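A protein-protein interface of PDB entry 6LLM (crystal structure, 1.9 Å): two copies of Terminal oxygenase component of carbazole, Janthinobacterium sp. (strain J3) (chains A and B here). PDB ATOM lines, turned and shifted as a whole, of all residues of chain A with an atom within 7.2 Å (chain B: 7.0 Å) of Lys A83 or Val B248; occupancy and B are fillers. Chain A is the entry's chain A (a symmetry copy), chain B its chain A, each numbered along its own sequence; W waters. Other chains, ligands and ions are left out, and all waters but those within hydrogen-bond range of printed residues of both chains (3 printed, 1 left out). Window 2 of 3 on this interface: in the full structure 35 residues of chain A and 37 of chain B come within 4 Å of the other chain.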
ATOM      1  N   LYS A  79      23.723 -27.036 -37.387  1.00  0.00           N
ATOM      2  CA  LYS A  79      23.305 -27.412 -36.048  1.00  0.00           C
ATOM      3  C   LYS A  79      22.714 -26.169 -35.371  1.00  0.00           C
ATOM      4  O   LYS A  79      23.434 -25.267 -34.950  1.00  0.00           O
ATOM      5  CB  LYS A  79      24.477 -27.944 -35.233  1.00  0.00           C
ATOM      6  CG  LYS A  79      24.166 -28.376 -33.810  1.00  0.00           C
ATOM      7  CD  LYS A  79      25.420 -28.848 -33.089  1.00  0.00           C
ATOM      8  CE  LYS A  79      25.233 -29.233 -31.624  1.00  0.00           C
ATOM      9  NZ  LYS A  79      24.790 -28.083 -30.767  1.00  0.00           N
ATOM     10  N   VAL A  80      21.390 -26.143 -35.301  1.00  0.00           N
ATOM     11  CA  VAL A  80      20.682 -25.005 -34.830  1.00  0.00           C
ATOM     12  C   VAL A  80      20.839 -24.977 -33.308  1.00  0.00           C
ATOM     13  O   VAL A  80      20.554 -25.977 -32.655  1.00  0.00           O
ATOM     14  CB  VAL A  80      19.199 -25.081 -35.254  1.00  0.00           C
ATOM     15  CG1 VAL A  80      18.367 -23.977 -34.592  1.00  0.00           C
ATOM     16  CG2 VAL A  80      19.059 -24.986 -36.760  1.00  0.00           C
ATOM     17  N   GLU A  81      21.177 -23.813 -32.755  1.00  0.00           N
ATOM     18  CA  GLU A  81      21.179 -23.620 -31.304  1.00  0.00           C
ATOM     19  C   GLU A  81      20.398 -22.331 -31.041  1.00  0.00           C
ATOM     20  O   GLU A  81      20.891 -21.210 -31.210  1.00  0.00           O
ATOM     21  CB  GLU A  81      22.594 -23.503 -30.771  1.00  0.00           C
ATOM     22  CG  GLU A  81      23.490 -24.698 -31.016  1.00  0.00           C
ATOM     23  CD  GLU A  81      24.834 -24.612 -30.275  1.00  0.00           C
ATOM     24  OE1 GLU A  81      25.074 -23.603 -29.547  1.00  0.00           O
ATOM     25  OE2 GLU A  81      25.681 -25.523 -30.448  1.00  0.00           O
ATOM     26  N   CYS A  82      19.127 -22.455 -30.735  1.00  0.00           N
ATOM     27  CA  CYS A  82      18.349 -21.281 -30.297  1.00  0.00           C
ATOM     28  C   CYS A  82      18.282 -21.372 -28.779  1.00  0.00           C
ATOM     29  O   CYS A  82      17.588 -22.253 -28.242  1.00  0.00           O
ATOM     30  CB  CYS A  82      16.982 -21.290 -30.956  1.00  0.00           C
ATOM     31  SG  CYS A  82      17.026 -20.970 -32.742  1.00  0.00           S
ATOM     32  N   LYS A  83      19.077 -20.529 -28.108  1.00  0.00           N
ATOM     33  CA  LYS A  83      19.258 -20.649 -26.650  1.00  0.00           C
ATOM     34  C   LYS A  83      18.434 -19.604 -25.888  1.00  0.00           C
ATOM     35  O   LYS A  83      18.360 -19.687 -24.656  1.00  0.00           O
ATOM     36  CB  LYS A  83      20.747 -20.533 -26.335  1.00  0.00           C
ATOM     37  CG  LYS A  83      21.608 -21.521 -27.097  1.00  0.00           C
ATOM     38  CD  LYS A  83      23.083 -21.379 -26.822  1.00  0.00           C
ATOM     39  CE  LYS A  83      23.783 -22.601 -26.255  1.00  0.00           C
ATOM     40  NZ  LYS A  83      23.348 -23.860 -26.902  1.00  0.00           N
ATOM     41  N   THR A  84      17.860 -18.611 -26.580  1.00  0.00           N
ATOM     42  CA  THR A  84      16.875 -17.706 -26.016  1.00  0.00           C
ATOM     43  C   THR A  84      15.861 -17.517 -27.109  1.00  0.00           C
ATOM     44  O   THR A  84      16.134 -17.768 -28.286  1.00  0.00           O
ATOM     45  CB  THR A  84      17.385 -16.340 -25.499  1.00  0.00           C
ATOM     46  OG1 THR A  84      17.702 -15.434 -26.568  1.00  0.00           O
ATOM     47  CG2 THR A  84      18.609 -16.447 -24.610  1.00  0.00           C
ATOM     48  N   LYS A  85      14.655 -17.151 -26.717  1.00  0.00           N
ATOM     49  CA  LYS A  85      13.615 -17.062 -27.670  1.00  0.00           C
ATOM     50  C   LYS A  85      13.967 -16.052 -28.777  1.00  0.00           C
ATOM     51  O   LYS A  85      13.510 -16.205 -29.906  1.00  0.00           O
ATOM     52  CB  LYS A  85      12.395 -16.574 -26.889  1.00  0.00           C
ATOM     53  CG  LYS A  85      11.157 -16.242 -27.687  1.00  0.00           C
ATOM     54  CD  LYS A  85      10.006 -15.967 -26.758  1.00  0.00           C
ATOM     55  CE  LYS A  85       9.493 -17.235 -26.115  1.00  0.00           C
ATOM     56  NZ  LYS A  85       8.093 -17.050 -25.652  1.00  0.00           N
ATOM     57  N   SER A  86      14.651 -14.955 -28.420  1.00  0.00           N
ATOM     58  CA  SER A  86      14.939 -13.867 -29.325  1.00  0.00           C
ATOM     59  C   SER A  86      16.145 -14.135 -30.261  1.00  0.00           C
ATOM     60  O   SER A  86      16.446 -13.250 -31.095  1.00  0.00           O
ATOM     61  CB  SER A  86      15.145 -12.588 -28.558  1.00  0.00           C
ATOM     62  OG  SER A  86      16.249 -12.684 -27.694  1.00  0.00           O
ATOM     63  N   THR A  87      16.916 -15.195 -30.018  1.00  0.00           N
ATOM     64  CA  THR A  87      18.196 -15.327 -30.655  1.00  0.00           C
ATOM     65  C   THR A  87      18.452 -16.703 -31.283  1.00  0.00           C
ATOM     66  O   THR A  87      17.826 -17.690 -31.015  1.00  0.00           O
ATOM     67  CB  THR A  87      19.374 -15.001 -29.728  1.00  0.00           C
ATOM     68  OG1 THR A  87      19.378 -15.970 -28.686  1.00  0.00           O
ATOM     69  CG2 THR A  87      19.304 -13.590 -29.173  1.00  0.00           C
ATOM     70  N   ILE A  88      19.477 -16.721 -32.145  1.00  0.00           N
ATOM     71  CA  ILE A  88      20.095 -17.966 -32.591  1.00  0.00           C
ATOM     72  C   ILE A  88      21.590 -17.800 -32.423  1.00  0.00           C
ATOM     73  O   ILE A  88      22.153 -16.763 -32.721  1.00  0.00           O
ATOM     74  CB  ILE A  88      19.719 -18.321 -34.069  1.00  0.00           C
ATOM     75  CG1 ILE A  88      20.397 -19.621 -34.539  1.00  0.00           C
ATOM     76  CG2 ILE A  88      20.020 -17.166 -35.023  1.00  0.00           C
ATOM     77  CD1 ILE A  88      19.754 -20.189 -35.868  1.00  0.00           C
ATOM     78  N   THR A  89      22.241 -18.893 -32.018  1.00  0.00           N
ATOM     79  CA  THR A  89      23.658 -18.940 -31.772  1.00  0.00           C
ATOM     80  C   THR A  89      24.347 -19.862 -32.811  1.00  0.00           C
ATOM     81  O   THR A  89      24.011 -21.041 -32.921  1.00  0.00           O
ATOM     82  CB  THR A  89      23.891 -19.473 -30.354  1.00  0.00           C
ATOM     83  OG1 THR A  89      23.450 -18.506 -29.387  1.00  0.00           O
ATOM     84  CG2 THR A  89      25.330 -19.762 -30.084  1.00  0.00           C
ATOM     85  N   CYS A  90      25.316 -19.339 -33.545  1.00  0.00           N
ATOM     86  CA  CYS A  90      26.064 -20.197 -34.440  1.00  0.00           C
ATOM     87  C   CYS A  90      26.737 -21.313 -33.636  1.00  0.00           C
ATOM     88  O   CYS A  90      27.342 -21.069 -32.592  1.00  0.00           O
ATOM     89  CB  CYS A  90      27.136 -19.405 -35.175  1.00  0.00           C
ATOM     90  SG  CYS A  90      28.070 -20.368 -36.401  1.00  0.00           S
ATOM     91  N   ALA A  94      29.847 -19.547 -31.666  1.00  0.00           N
ATOM     92  CA  ALA A  94      28.754 -19.030 -30.850  1.00  0.00           C
ATOM     93  C   ALA A  94      28.516 -17.525 -31.060  1.00  0.00           C
ATOM     94  O   ALA A  94      28.011 -16.885 -30.147  1.00  0.00           O
ATOM     95  CB  ALA A  94      28.987 -19.343 -29.378  1.00  0.00           C
ATOM     96  N   THR A  96      26.023 -14.842 -31.834  1.00  0.00           N
ATOM     97  CA  THR A  96      24.627 -14.913 -31.515  1.00  0.00           C
ATOM     98  C   THR A  96      23.927 -13.698 -32.107  1.00  0.00           C
ATOM     99  O   THR A  96      24.345 -12.525 -31.872  1.00  0.00           O
ATOM    100  CB  THR A  96      24.426 -14.998 -29.986  1.00  0.00           C
ATOM    101  OG1 THR A  96      25.054 -16.213 -29.549  1.00  0.00           O
ATOM    102  CG2 THR A  96      22.968 -15.029 -29.589  1.00  0.00           C
ATOM    103  N   LEU A 108      29.303 -16.050 -27.376  1.00  0.00           N
ATOM    104  CA  LEU A 108      29.513 -16.889 -26.144  1.00  0.00           C
ATOM    105  C   LEU A 108      30.998 -17.202 -25.944  1.00  0.00           C
ATOM    106  O   LEU A 108      31.436 -17.282 -24.807  1.00  0.00           O
ATOM    107  CB  LEU A 108      28.715 -18.179 -26.225  1.00  0.00           C
ATOM    108  CG  LEU A 108      27.256 -18.095 -25.818  1.00  0.00           C
ATOM    109  CD1 LEU A 108      26.563 -16.893 -26.350  1.00  0.00           C
ATOM    110  CD2 LEU A 108      26.509 -19.387 -26.105  1.00  0.00           C
ATOM    111  N   TYR B 185      34.266 -24.500 -28.621  1.00  0.00           N
ATOM    112  CA  TYR B 185      32.831 -24.493 -28.422  1.00  0.00           C
ATOM    113  C   TYR B 185      32.166 -25.743 -29.000  1.00  0.00           C
ATOM    114  O   TYR B 185      31.151 -26.264 -28.481  1.00  0.00           O
ATOM    115  CB  TYR B 185      32.270 -23.193 -29.021  1.00  0.00           C
ATOM    116  CG  TYR B 185      30.800 -23.006 -28.775  1.00  0.00           C
ATOM    117  CD1 TYR B 185      30.354 -22.646 -27.519  1.00  0.00           C
ATOM    118  CD2 TYR B 185      29.863 -23.201 -29.764  1.00  0.00           C
ATOM    119  CE1 TYR B 185      29.014 -22.494 -27.258  1.00  0.00           C
ATOM    120  CE2 TYR B 185      28.512 -23.083 -29.510  1.00  0.00           C
ATOM    121  CZ  TYR B 185      28.087 -22.702 -28.245  1.00  0.00           C
ATOM    122  OH  TYR B 185      26.765 -22.612 -27.964  1.00  0.00           O
ATOM    123  N   LYS B 188      31.931 -29.004 -26.774  1.00  0.00           N
ATOM    124  CA  LYS B 188      31.378 -28.866 -25.421  1.00  0.00           C
ATOM    125  C   LYS B 188      30.527 -30.070 -25.000  1.00  0.00           C
ATOM    126  O   LYS B 188      30.370 -30.337 -23.792  1.00  0.00           O
ATOM    127  CB  LYS B 188      30.538 -27.600 -25.292  1.00  0.00           C
ATOM    128  CG  LYS B 188      29.313 -27.563 -26.181  1.00  0.00           C
ATOM    129  CD  LYS B 188      28.765 -26.149 -26.238  1.00  0.00           C
ATOM    130  CE  LYS B 188      27.482 -26.030 -27.001  1.00  0.00           C
ATOM    131  NZ  LYS B 188      27.698 -26.158 -28.462  1.00  0.00           N
ATOM    132  N   LEU B 202      34.387 -22.830 -22.772  1.00  0.00           N
ATOM    133  CA  LEU B 202      33.607 -22.539 -23.971  1.00  0.00           C
ATOM    134  C   LEU B 202      34.435 -21.719 -24.965  1.00  0.00           C
ATOM    135  O   LEU B 202      34.105 -21.711 -26.125  1.00  0.00           O
ATOM    136  CB  LEU B 202      32.369 -21.757 -23.569  1.00  0.00           C
ATOM    137  CG  LEU B 202      31.344 -22.553 -22.756  1.00  0.00           C
ATOM    138  CD1 LEU B 202      30.102 -21.693 -22.558  1.00  0.00           C
ATOM    139  CD2 LEU B 202      30.952 -23.876 -23.405  1.00  0.00           C
ATOM    140  N   GLU B 240      31.128 -19.508 -18.676  1.00  0.00           N
ATOM    141  CA  GLU B 240      29.770 -19.198 -18.651  1.00  0.00           C
ATOM    142  C   GLU B 240      29.440 -18.420 -19.921  1.00  0.00           C
ATOM    143  O   GLU B 240      29.951 -17.332 -20.131  1.00  0.00           O
ATOM    144  CB  GLU B 240      29.416 -18.357 -17.437  1.00  0.00           C
ATOM    145  CG  GLU B 240      29.423 -19.173 -16.169  1.00  0.00           C
ATOM    146  CD  GLU B 240      29.303 -18.320 -14.908  1.00  0.00           C
ATOM    147  OE1 GLU B 240      29.087 -17.089 -15.021  1.00  0.00           O
ATOM    148  OE2 GLU B 240      29.441 -18.893 -13.825  1.00  0.00           O
ATOM    149  N   GLY B 241      28.549 -18.993 -20.730  1.00  0.00           N
ATOM    150  CA  GLY B 241      28.078 -18.327 -21.917  1.00  0.00           C
ATOM    151  C   GLY B 241      26.774 -17.609 -21.651  1.00  0.00           C
ATOM    152  O   GLY B 241      25.823 -18.248 -21.254  1.00  0.00           O
ATOM    153  N   THR B 242      26.746 -16.302 -21.934  1.00  0.00           N
ATOM    154  CA  THR B 242      25.629 -15.463 -21.659  1.00  0.00           C
ATOM    155  C   THR B 242      25.075 -14.889 -22.957  1.00  0.00           C
ATOM    156  O   THR B 242      25.831 -14.556 -23.871  1.00  0.00           O
ATOM    157  CB  THR B 242      25.993 -14.329 -20.693  1.00  0.00           C
ATOM    158  OG1 THR B 242      27.029 -13.550 -21.283  1.00  0.00           O
ATOM    159  CG2 THR B 242      26.466 -14.861 -19.368  1.00  0.00           C
ATOM    160  N   ILE B 243      23.761 -14.738 -22.958  1.00  0.00           N
ATOM    161  CA  ILE B 243      23.035 -13.975 -23.912  1.00  0.00           C
ATOM    162  C   ILE B 243      22.184 -12.948 -23.177  1.00  0.00           C
ATOM    163  O   ILE B 243      21.324 -13.352 -22.357  1.00  0.00           O
ATOM    164  CB  ILE B 243      22.185 -14.900 -24.795  1.00  0.00           C
ATOM    165  CG1 ILE B 243      23.077 -15.876 -25.567  1.00  0.00           C
ATOM    166  CG2 ILE B 243      21.361 -14.033 -25.724  1.00  0.00           C
ATOM    167  CD1 ILE B 243      22.252 -16.886 -26.383  1.00  0.00           C
ATOM    168  N   GLY B 245      23.202 -11.124 -20.865  1.00  0.00           N
ATOM    169  CA  GLY B 245      23.573 -11.293 -19.482  1.00  0.00           C
ATOM    170  C   GLY B 245      23.110 -12.594 -18.839  1.00  0.00           C
ATOM    171  O   GLY B 245      23.566 -12.870 -17.759  1.00  0.00           O
ATOM    172  N   GLU B 246      22.235 -13.374 -19.497  1.00  0.00           N
ATOM    173  CA  GLU B 246      21.700 -14.601 -18.942  1.00  0.00           C
ATOM    174  C   GLU B 246      22.593 -15.792 -19.250  1.00  0.00           C
ATOM    175  O   GLU B 246      22.937 -16.021 -20.440  1.00  0.00           O
ATOM    176  CB  GLU B 246      20.335 -14.886 -19.536  1.00  0.00           C
ATOM    177  CG  GLU B 246      19.738 -16.162 -18.993  1.00  0.00           C
ATOM    178  CD  GLU B 246      18.232 -16.145 -19.103  1.00  0.00           C
ATOM    179  OE1 GLU B 246      17.636 -15.097 -18.716  1.00  0.00           O
ATOM    180  OE2 GLU B 246      17.667 -17.149 -19.593  1.00  0.00           O
ATOM    181  N   VAL B 247      22.930 -16.599 -18.233  1.00  0.00           N
ATOM    182  CA  VAL B 247      23.785 -17.756 -18.491  1.00  0.00           C
ATOM    183  C   VAL B 247      22.949 -18.821 -19.199  1.00  0.00           C
ATOM    184  O   VAL B 247      21.928 -19.197 -18.684  1.00  0.00           O
ATOM    185  CB  VAL B 247      24.434 -18.312 -17.211  1.00  0.00           C
ATOM    186  CG1 VAL B 247      25.218 -19.578 -17.526  1.00  0.00           C
ATOM    187  CG2 VAL B 247      25.337 -17.270 -16.575  1.00  0.00           C
ATOM    188  N   VAL B 248      23.325 -19.218 -20.423  1.00  0.00           N
ATOM    189  CA  VAL B 248      22.567 -20.180 -21.168  1.00  0.00           C
ATOM    190  C   VAL B 248      23.375 -21.462 -21.427  1.00  0.00           C
ATOM    191  O   VAL B 248      22.796 -22.421 -21.837  1.00  0.00           O
ATOM    192  CB  VAL B 248      22.047 -19.624 -22.520  1.00  0.00           C
ATOM    193  CG1 VAL B 248      21.010 -18.528 -22.361  1.00  0.00           C
ATOM    194  CG2 VAL B 248      23.177 -19.191 -23.419  1.00  0.00           C
ATOM    195  N   ARG B 249      24.678 -21.470 -21.172  1.00  0.00           N
ATOM    196  CA  ARG B 249      25.485 -22.611 -21.365  1.00  0.00           C
ATOM    197  C   ARG B 249      26.710 -22.483 -20.475  1.00  0.00           C
ATOM    198  O   ARG B 249      27.266 -21.387 -20.299  1.00  0.00           O
ATOM    199  CB  ARG B 249      25.970 -22.696 -22.833  1.00  0.00           C
ATOM    200  CG  ARG B 249      26.875 -23.884 -23.109  1.00  0.00           C
ATOM    201  CD  ARG B 249      26.191 -25.228 -22.976  1.00  0.00           C
ATOM    202  NE  ARG B 249      27.142 -26.338 -22.752  1.00  0.00           N
ATOM    203  CZ  ARG B 249      26.988 -27.554 -23.267  1.00  0.00           C
ATOM    204  NH1 ARG B 249      26.061 -27.769 -24.199  1.00  0.00           N
ATOM    205  NH2 ARG B 249      27.797 -28.516 -22.890  1.00  0.00           N
ATOM    206  N   GLU B 250      27.183 -23.615 -19.970  1.00  0.00           N
ATOM    207  CA  GLU B 250      28.393 -23.626 -19.216  1.00  0.00           C
ATOM    208  C   GLU B 250      29.402 -24.602 -19.811  1.00  0.00           C
ATOM    209  O   GLU B 250      29.050 -25.484 -20.531  1.00  0.00           O
ATOM    210  CB  GLU B 250      28.132 -24.054 -17.770  1.00  0.00           C
ATOM    211  CG  GLU B 250      27.288 -23.058 -17.004  1.00  0.00           C
ATOM    212  CD  GLU B 250      27.318 -23.344 -15.508  1.00  0.00           C
ATOM    213  OE1 GLU B 250      28.054 -22.642 -14.764  1.00  0.00           O
ATOM    214  OE2 GLU B 250      26.668 -24.320 -15.119  1.00  0.00           O
HETATM  215  O   HOH W   1      29.985 -15.807 -22.909  1.00  0.00           O
HETATM  216  O   HOH W   2      28.267 -26.680 -31.447  1.00  0.00           O
HETATM  217  O   HOH W   3      24.086 -26.273 -25.595  1.00  0.00           O
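NZ of Lys B188 lies within salt-bridge range of OE2 of Glu A81, at 2.9 Å. The side-chain hydroxyl (OH) of Tyr B185 is in hydrogen-bond range of the side-chain carboxylate (OE1) of Glu A81, 2.5 Å away.
O of Lys B188 sits at hydrogen-bond distance from NH2 of Arg B249 (3.3 Å). The backbone carbonyl oxygen (O) of Ala A94 is in hydrogen-bond range of the side-chain hydroxyl (OG1) of Thr A96, at 3.1 Å. The side-chain hydroxyl of Thr A89 is in hydrogen-bond range of the side-chain hydroxyl of Thr A96 (2.8 Å). The side-chain amino group of Lys A79 lies within salt-bridge range of the side-chain carboxylate of Glu A81, at 2.7 Å. The side-chain sulfur (SG) of Cys A82 lies close to the backbone carbonyl oxygen (O) of Thr A87 (3.8 Å). The backbone carbonyl oxygen of Arg B249 lies within hydrogen-bond range of the backbone NH of Gly B241 (2.8 Å).
Among the printed residues, merely in contact across the chains: Lys A83 with Tyr B185, Lys A83 with Ile B243, Lys A83 with Val B248, Thr A84 with Ile B243, Thr A84 with Val B248, Thr A87 with Ile B243, Thr A89 with Tyr B185, Thr A89 with Ile B243, Cys A90 with Tyr B185, Ala A94 with Tyr B185, Thr A96 with Ile B243, Leu A108 with Tyr B185, Leu A108 with Gly B241, Leu A108 with Thr B242 and Leu A108 with Ile B243.
Val B248 touches two residues of chain A. Printed residues of chain B within 4 Å of Thr A87: Ile B243 (3.8 Å). Printed residues of chain B within 4 Å of Cys A90: Tyr B185 (3.9 Å). Of the printed residues of chain B, Thr A96 touches Ile B243 (3.8 Å). Printed residues of chain B within 4 Å of Ala A94: Tyr B185. Printed residues of chain B within 4 Å of Glu A81: Tyr B185 and Lys B188. The nearest residue of chain A that does not touch Val B248 is Leu A108 (4.3 Å).
Hydrophobic or aromatic side chains of chain A that line the printed part of chain B: Ala A94 and Leu A108. Printed residues of chain B that touch a printed residue of chain A: Tyr B185, Lys B188, Gly B241, Thr B242, Ile B243 and Val B248. Among the printed residues, Asp or Glu carboxylates within 4 Å of a Lys or Arg side-chain nitrogen of the other chain: Glu A81 with Lys B188 (2.9 Å).
No position is printed for both chains. Of the 17 pairs that touch across the chains among the printed residues, none has its exchanged pair printed and touching as well.
Water W1 lies within hydrogen-bond range of the backbone carbonyl oxygen of Leu A108 (2.8 Å), the backbone carbonyl oxygen of Glu B240 (3.2 Å) and the backbone NH of Thr B242 (3.4 Å). Water W3 bridges the side-chain amino group of Lys A83 and the guanidinium group of Arg B249. Water W2 lies within hydrogen-bond range of the side-chain carboxylate of Glu A81 and the side-chain amino group of Lys B188.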
